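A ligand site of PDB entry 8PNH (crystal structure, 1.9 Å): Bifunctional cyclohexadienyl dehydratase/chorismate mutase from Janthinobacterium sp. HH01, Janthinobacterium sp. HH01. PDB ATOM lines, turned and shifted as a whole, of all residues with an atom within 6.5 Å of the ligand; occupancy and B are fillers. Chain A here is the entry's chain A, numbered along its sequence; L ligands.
NH1 of Arg 276 lies within salt-bridge range of O3 of the ligand.
The guanidinium group (NH2) of Arg 362 lies within salt-bridge range of an oxygen (O5) of the ligand, at 2.8 Å.
The side-chain amide nitrogen (NE2) of Gln 336 is in hydrogen-bond range of an oxygen (O2) of the ligand.
An oxygen (O6) of the ligand is in salt-bridge range of the side-chain amino group (NZ) of Lys 287 (3.0 Å).
The side-chain carboxylate (OE2) of Glu 300 is in hydrogen-bond range of an oxygen (O1) of the ligand, 3.0 Å away.
N of Asp 296 sits at hydrogen-bond distance from O1 of the ligand, at 3.1 Å.
An oxygen (O4) of the ligand lies within salt-bridge range of the guanidinium group (NH1) of Arg 299 (3.4 Å).
O1 of the ligand lies within hydrogen-bond range of O of Ile 294 (3.5 Å).
OG1 of Thr 369 lies within hydrogen-bond range of NE of Arg 276 (3.4 Å).
The backbone NH of Arg 362 lies within hydrogen-bond range of the backbone carbonyl oxygen of Leu 357, 3.0 Å away.
The side-chain amide oxygen (OE1) of Gln 336 sits at hydrogen-bond distance from the side-chain amino group (NZ) of Lys 287 (2.9 Å).
The side-chain amide nitrogen (NE2) of Gln 336 lies within hydrogen-bond range of the side-chain hydroxyl (OG) of Ser 332 (3.0 Å).
The backbone carbonyl oxygen of Ile 294 sits at hydrogen-bond distance from the side-chain amino group of Lys 287, 2.7 Å away.
OE2 of Glu 300 lies within salt-bridge range of NZ of Lys 333 (2.9 Å).
The side-chain carboxylate (OD1) of Asp 296 is in hydrogen-bond range of the backbone NH (N) of Arg 299 (3.4 Å).
NZ of Lys 333 lies within salt-bridge range of OE2 of Glu 330, at 3.0 Å.
Val 283 touches the ligand.
Glu 295 touches the ligand (CA to O1, 3.9 Å).
Val 303 touches the ligand.
Ser 332 touches the ligand.
Lys 333 touches the ligand (CD to O1, 3.9 Å).
Hydrophobic or aromatic side chains that line the ligand: Val 283 and Val 303.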
ATOM      1  N   ARG A 276     -13.434  13.421  37.067  1.00  0.00           N
ATOM      2  CA  ARG A 276     -13.404  14.198  35.835  1.00  0.00           C
ATOM      3  C   ARG A 276     -13.802  13.292  34.670  1.00  0.00           C
ATOM      4  O   ARG A 276     -14.614  13.648  33.823  1.00  0.00           O
ATOM      5  CB  ARG A 276     -12.037  14.869  35.666  1.00  0.00           C
ATOM      6  CG  ARG A 276     -12.001  16.018  34.661  1.00  0.00           C
ATOM      7  CD  ARG A 276     -10.593  16.511  34.373  1.00  0.00           C
ATOM      8  NE  ARG A 276     -10.604  17.789  33.635  1.00  0.00           N
ATOM      9  CZ  ARG A 276     -10.981  17.941  32.368  1.00  0.00           C
ATOM     10  NH1 ARG A 276     -11.164  16.891  31.573  1.00  0.00           N
ATOM     11  NH2 ARG A 276     -11.148  19.158  31.873  1.00  0.00           N
ATOM     12  N   VAL A 283     -21.069  14.939  29.559  1.00  0.00           N
ATOM     13  CA  VAL A 283     -20.646  15.683  28.386  1.00  0.00           C
ATOM     14  C   VAL A 283     -21.187  15.008  27.121  1.00  0.00           C
ATOM     15  O   VAL A 283     -21.688  15.697  26.235  1.00  0.00           O
ATOM     16  CB  VAL A 283     -19.108  15.802  28.299  1.00  0.00           C
ATOM     17  CG1 VAL A 283     -18.655  16.397  26.972  1.00  0.00           C
ATOM     18  CG2 VAL A 283     -18.510  16.592  29.451  1.00  0.00           C
ATOM     19  N   LYS A 287     -23.789  16.544  24.319  1.00  0.00           N
ATOM     20  CA  LYS A 287     -23.383  16.665  22.919  1.00  0.00           C
ATOM     21  C   LYS A 287     -24.286  15.858  21.963  1.00  0.00           C
ATOM     22  O   LYS A 287     -24.561  16.318  20.865  1.00  0.00           O
ATOM     23  CB  LYS A 287     -21.915  16.258  22.746  1.00  0.00           C
ATOM     24  CG  LYS A 287     -20.912  17.243  23.354  1.00  0.00           C
ATOM     25  CD  LYS A 287     -19.513  16.867  23.034  1.00  0.00           C
ATOM     26  CE  LYS A 287     -18.474  17.786  23.614  1.00  0.00           C
ATOM     27  NZ  LYS A 287     -17.133  17.212  23.383  1.00  0.00           N
ATOM     28  N   PRO A 293     -19.786  17.908  17.751  1.00  0.00           N
ATOM     29  CA  PRO A 293     -18.586  17.079  17.635  1.00  0.00           C
ATOM     30  C   PRO A 293     -17.948  16.821  19.003  1.00  0.00           C
ATOM     31  O   PRO A 293     -17.932  17.667  19.895  1.00  0.00           O
ATOM     32  CB  PRO A 293     -17.606  17.853  16.760  1.00  0.00           C
ATOM     33  CG  PRO A 293     -18.463  18.889  16.057  1.00  0.00           C
ATOM     34  CD  PRO A 293     -19.707  19.092  16.908  1.00  0.00           C
ATOM     35  N   ILE A 294     -17.434  15.605  19.158  1.00  0.00           N
ATOM     36  CA  ILE A 294     -16.724  15.258  20.364  1.00  0.00           C
ATOM     37  C   ILE A 294     -15.469  16.128  20.486  1.00  0.00           C
ATOM     38  O   ILE A 294     -15.197  16.632  21.574  1.00  0.00           O
ATOM     39  CB  ILE A 294     -16.400  13.738  20.378  1.00  0.00           C
ATOM     40  CG1 ILE A 294     -17.671  12.914  20.658  1.00  0.00           C
ATOM     41  CG2 ILE A 294     -15.302  13.430  21.388  1.00  0.00           C
ATOM     42  CD1 ILE A 294     -17.511  11.406  20.312  1.00  0.00           C
ATOM     43  N   GLU A 295     -14.682  16.249  19.431  1.00  0.00           N
ATOM     44  CA  GLU A 295     -13.378  16.904  19.539  1.00  0.00           C
ATOM     45  C   GLU A 295     -13.565  18.392  19.248  1.00  0.00           C
ATOM     46  O   GLU A 295     -14.145  18.745  18.216  1.00  0.00           O
ATOM     47  CB  GLU A 295     -12.334  16.281  18.611  1.00  0.00           C
ATOM     48  CG  GLU A 295     -10.941  16.869  18.733  1.00  0.00           C
ATOM     49  CD  GLU A 295      -9.867  16.055  18.045  1.00  0.00           C
ATOM     50  OE1 GLU A 295      -9.645  16.284  16.851  1.00  0.00           O
ATOM     51  OE2 GLU A 295      -9.279  15.137  18.671  1.00  0.00           O
ATOM     52  N   ASP A 296     -13.106  19.236  20.176  1.00  0.00           N
ATOM     53  CA  ASP A 296     -13.241  20.685  20.096  1.00  0.00           C
ATOM     54  C   ASP A 296     -11.901  21.264  20.545  1.00  0.00           C
ATOM     55  O   ASP A 296     -11.748  21.617  21.710  1.00  0.00           O
ATOM     56  CB  ASP A 296     -14.410  21.140  20.976  1.00  0.00           C
ATOM     57  CG  ASP A 296     -14.634  22.648  21.035  1.00  0.00           C
ATOM     58  OD1 ASP A 296     -13.874  23.376  20.366  1.00  0.00           O
ATOM     59  OD2 ASP A 296     -15.577  23.076  21.758  1.00  0.00           O
ATOM     60  N   LEU A 297     -10.944  21.335  19.606  1.00  0.00           N
ATOM     61  CA  LEU A 297      -9.560  21.697  19.907  1.00  0.00           C
ATOM     62  C   LEU A 297      -9.442  23.161  20.362  1.00  0.00           C
ATOM     63  O   LEU A 297      -8.376  23.572  20.820  1.00  0.00           O
ATOM     64  CB  LEU A 297      -8.673  21.429  18.686  1.00  0.00           C
ATOM     65  CG  LEU A 297      -7.633  20.314  18.828  1.00  0.00           C
ATOM     66  CD1 LEU A 297      -6.667  20.601  19.963  1.00  0.00           C
ATOM     67  CD2 LEU A 297      -8.291  18.958  19.023  1.00  0.00           C
ATOM     68  N   ARG A 299     -11.797  24.594  22.729  1.00  0.00           N
ATOM     69  CA  ARG A 299     -12.067  24.492  24.149  1.00  0.00           C
ATOM     70  C   ARG A 299     -10.909  23.736  24.836  1.00  0.00           C
ATOM     71  O   ARG A 299     -10.650  23.999  26.009  1.00  0.00           O
ATOM     72  CB  ARG A 299     -13.439  23.865  24.377  1.00  0.00           C
ATOM     73  CG  ARG A 299     -14.091  24.211  25.704  1.00  0.00           C
ATOM     74  CD  ARG A 299     -13.935  23.128  26.749  1.00  0.00           C
ATOM     75  NE  ARG A 299     -14.294  23.617  28.069  1.00  0.00           N
ATOM     76  CZ  ARG A 299     -14.260  22.896  29.186  1.00  0.00           C
ATOM     77  NH1 ARG A 299     -14.188  21.572  29.123  1.00  0.00           N
ATOM     78  NH2 ARG A 299     -14.329  23.492  30.360  1.00  0.00           N
ATOM     79  N   GLU A 300     -10.203  22.873  24.081  1.00  0.00           N
ATOM     80  CA  GLU A 300      -9.023  22.159  24.555  1.00  0.00           C
ATOM     81  C   GLU A 300      -7.882  23.140  24.840  1.00  0.00           C
ATOM     82  O   GLU A 300      -7.174  22.980  25.841  1.00  0.00           O
ATOM     83  CB  GLU A 300      -8.519  21.116  23.558  1.00  0.00           C
ATOM     84  CG  GLU A 300      -9.407  19.878  23.432  1.00  0.00           C
ATOM     85  CD  GLU A 300      -8.907  18.733  22.552  1.00  0.00           C
ATOM     86  OE1 GLU A 300      -7.696  18.719  22.182  1.00  0.00           O
ATOM     87  OE2 GLU A 300      -9.724  17.836  22.235  1.00  0.00           O
ATOM     88  N   VAL A 303      -8.606  25.099  27.915  1.00  0.00           N
ATOM     89  CA  VAL A 303      -8.438  24.221  29.075  1.00  0.00           C
ATOM     90  C   VAL A 303      -6.970  24.129  29.429  1.00  0.00           C
ATOM     91  O   VAL A 303      -6.635  24.273  30.588  1.00  0.00           O
ATOM     92  CB  VAL A 303      -9.054  22.817  28.852  1.00  0.00           C
ATOM     93  CG1 VAL A 303      -8.562  21.800  29.869  1.00  0.00           C
ATOM     94  CG2 VAL A 303     -10.582  22.879  28.875  1.00  0.00           C
ATOM     95  N   GLN A 328      -5.790  13.749  30.072  1.00  0.00           N
ATOM     96  CA  GLN A 328      -7.135  13.785  30.634  1.00  0.00           C
ATOM     97  C   GLN A 328      -8.151  14.111  29.510  1.00  0.00           C
ATOM     98  O   GLN A 328      -9.272  13.636  29.513  1.00  0.00           O
ATOM     99  CB  GLN A 328      -7.232  14.830  31.776  1.00  0.00           C
ATOM    100  CG  GLN A 328      -6.280  14.627  32.974  1.00  0.00           C
ATOM    101  CD  GLN A 328      -6.057  13.161  33.324  1.00  0.00           C
ATOM    102  OE1 GLN A 328      -6.987  12.439  33.684  1.00  0.00           O
ATOM    103  NE2 GLN A 328      -4.845  12.676  33.120  1.00  0.00           N
ATOM    104  N   ILE A 329      -7.810  15.049  28.641  1.00  0.00           N
ATOM    105  CA  ILE A 329      -8.691  15.445  27.536  1.00  0.00           C
ATOM    106  C   ILE A 329      -8.888  14.270  26.567  1.00  0.00           C
ATOM    107  O   ILE A 329      -9.994  14.026  26.093  1.00  0.00           O
ATOM    108  CB  ILE A 329      -8.105  16.701  26.853  1.00  0.00           C
ATOM    109  CG1 ILE A 329      -8.195  17.921  27.776  1.00  0.00           C
ATOM    110  CG2 ILE A 329      -8.707  16.977  25.472  1.00  0.00           C
ATOM    111  CD1 ILE A 329      -7.347  19.076  27.308  1.00  0.00           C
ATOM    112  N   GLU A 330      -7.807  13.537  26.263  1.00  0.00           N
ATOM    113  CA  GLU A 330      -7.887  12.393  25.351  1.00  0.00           C
ATOM    114  C   GLU A 330      -8.680  11.258  25.968  1.00  0.00           C
ATOM    115  O   GLU A 330      -9.468  10.614  25.266  1.00  0.00           O
ATOM    116  CB  GLU A 330      -6.501  11.866  24.987  1.00  0.00           C
ATOM    117  CG  GLU A 330      -5.697  12.842  24.157  1.00  0.00           C
ATOM    118  CD  GLU A 330      -6.321  13.217  22.817  1.00  0.00           C
ATOM    119  OE1 GLU A 330      -6.937  12.333  22.188  1.00  0.00           O
ATOM    120  OE2 GLU A 330      -6.187  14.405  22.398  1.00  0.00           O
ATOM    121  N   SER A 332     -11.073  11.669  28.148  1.00  0.00           N
ATOM    122  CA  SER A 332     -12.460  12.101  28.054  1.00  0.00           C
ATOM    123  C   SER A 332     -13.103  11.820  26.678  1.00  0.00           C
ATOM    124  O   SER A 332     -14.256  11.413  26.585  1.00  0.00           O
ATOM    125  CB  SER A 332     -12.574  13.579  28.356  1.00  0.00           C
ATOM    126  OG  SER A 332     -13.924  14.006  28.162  1.00  0.00           O
ATOM    127  N   LYS A 333     -12.396  12.144  25.599  1.00  0.00           N
ATOM    128  CA  LYS A 333     -12.903  11.917  24.250  1.00  0.00           C
ATOM    129  C   LYS A 333     -13.077  10.425  24.007  1.00  0.00           C
ATOM    130  O   LYS A 333     -14.018  10.033  23.323  1.00  0.00           O
ATOM    131  CB  LYS A 333     -12.002  12.587  23.227  1.00  0.00           C
ATOM    132  CG  LYS A 333     -12.066  14.113  23.240  1.00  0.00           C
ATOM    133  CD  LYS A 333     -11.176  14.813  22.214  1.00  0.00           C
ATOM    134  CE  LYS A 333      -9.763  14.272  22.182  1.00  0.00           C
ATOM    135  NZ  LYS A 333      -8.866  15.179  21.426  1.00  0.00           N
ATOM    136  N   GLN A 336     -16.359   9.545  25.465  1.00  0.00           N
ATOM    137  CA  GLN A 336     -17.389  10.104  24.599  1.00  0.00           C
ATOM    138  C   GLN A 336     -17.545   9.270  23.321  1.00  0.00           C
ATOM    139  O   GLN A 336     -18.664   8.883  22.948  1.00  0.00           O
ATOM    140  CB  GLN A 336     -17.070  11.570  24.308  1.00  0.00           C
ATOM    141  CG  GLN A 336     -17.183  12.476  25.532  1.00  0.00           C
ATOM    142  CD  GLN A 336     -16.775  13.887  25.175  1.00  0.00           C
ATOM    143  OE1 GLN A 336     -17.360  14.521  24.304  1.00  0.00           O
ATOM    144  NE2 GLN A 336     -15.712  14.362  25.799  1.00  0.00           N
ATOM    145  N   LEU A 357     -24.273  21.609  29.424  1.00  0.00           N
ATOM    146  CA  LEU A 357     -22.830  21.465  29.207  1.00  0.00           C
ATOM    147  C   LEU A 357     -22.091  22.736  29.623  1.00  0.00           C
ATOM    148  O   LEU A 357     -21.356  22.740  30.616  1.00  0.00           O
ATOM    149  CB  LEU A 357     -22.569  21.128  27.735  1.00  0.00           C
ATOM    150  CG  LEU A 357     -21.102  21.038  27.317  1.00  0.00           C
ATOM    151  CD1 LEU A 357     -20.431  19.829  27.961  1.00  0.00           C
ATOM    152  CD2 LEU A 357     -20.976  20.960  25.799  1.00  0.00           C
ATOM    153  N   ARG A 362     -19.331  22.161  32.817  1.00  0.00           N
ATOM    154  CA  ARG A 362     -18.015  22.749  32.623  1.00  0.00           C
ATOM    155  C   ARG A 362     -17.514  23.427  33.906  1.00  0.00           C
ATOM    156  O   ARG A 362     -16.302  23.433  34.157  1.00  0.00           O
ATOM    157  CB  ARG A 362     -18.020  23.655  31.388  1.00  0.00           C
ATOM    158  CG  ARG A 362     -17.993  22.859  30.095  1.00  0.00           C
ATOM    159  CD  ARG A 362     -17.824  23.666  28.812  1.00  0.00           C
ATOM    160  NE  ARG A 362     -17.816  22.756  27.678  1.00  0.00           N
ATOM    161  CZ  ARG A 362     -17.581  23.130  26.424  1.00  0.00           C
ATOM    162  NH1 ARG A 362     -17.432  24.406  26.130  1.00  0.00           N
ATOM    163  NH2 ARG A 362     -17.501  22.219  25.472  1.00  0.00           N
ATOM    164  N   LEU A 365     -16.126  20.535  35.744  1.00  0.00           N
ATOM    165  CA  LEU A 365     -14.859  20.117  35.151  1.00  0.00           C
ATOM    166  C   LEU A 365     -13.754  21.060  35.642  1.00  0.00           C
ATOM    167  O   LEU A 365     -12.649  20.632  35.961  1.00  0.00           O
ATOM    168  CB  LEU A 365     -14.960  20.105  33.622  1.00  0.00           C
ATOM    169  CG  LEU A 365     -15.803  18.961  33.041  1.00  0.00           C
ATOM    170  CD1 LEU A 365     -16.042  19.151  31.561  1.00  0.00           C
ATOM    171  CD2 LEU A 365     -15.146  17.614  33.304  1.00  0.00           C
ATOM    172  N   THR A 369     -10.400  20.093  37.686  1.00  0.00           N
ATOM    173  CA  THR A 369      -9.112  20.548  37.187  1.00  0.00           C
ATOM    174  C   THR A 369      -8.285  21.200  38.295  1.00  0.00           C
ATOM    175  O   THR A 369      -7.108  20.868  38.473  1.00  0.00           O
ATOM    176  CB  THR A 369      -9.307  21.545  36.031  1.00  0.00           C
ATOM    177  OG1 THR A 369      -9.785  20.797  34.908  1.00  0.00           O
ATOM    178  CG2 THR A 369      -8.034  22.279  35.674  1.00  0.00           C
HETATM  179  C1  LIG L   1     -12.975  18.240  27.129  1.00  0.00           C
HETATM  180  C2  LIG L   1     -12.694  19.527  26.361  1.00  0.00           C
HETATM  181  C3  LIG L   1     -12.925  19.634  25.050  1.00  0.00           C
HETATM  182  C4  LIG L   1     -13.443  18.523  24.181  1.00  0.00           C
HETATM  183  O1  LIG L   1     -12.531  18.312  23.089  1.00  0.00           O
HETATM  184  C5  LIG L   1     -13.659  17.217  24.965  1.00  0.00           C
HETATM  185  C6  LIG L   1     -12.741  17.060  26.176  1.00  0.00           C
HETATM  186  O2  LIG L   1     -15.047  17.118  25.357  1.00  0.00           O
HETATM  187  C7  LIG L   1     -15.500  17.966  26.446  1.00  0.00           C
HETATM  188  C8  LIG L   1     -14.459  18.203  27.548  1.00  0.00           C
HETATM  189  C9  LIG L   1     -12.267  18.203  28.490  1.00  0.00           C
HETATM  190  O3  LIG L   1     -12.229  17.163  29.100  1.00  0.00           O
HETATM  191  O4  LIG L   1     -11.806  19.200  29.001  1.00  0.00           O
HETATM  192  C10 LIG L   1     -16.080  19.318  26.016  1.00  0.00           C
HETATM  193  O5  LIG L   1     -16.479  20.080  26.885  1.00  0.00           O
HETATM  194  O6  LIG L   1     -16.164  19.620  24.847  1.00  0.00           O
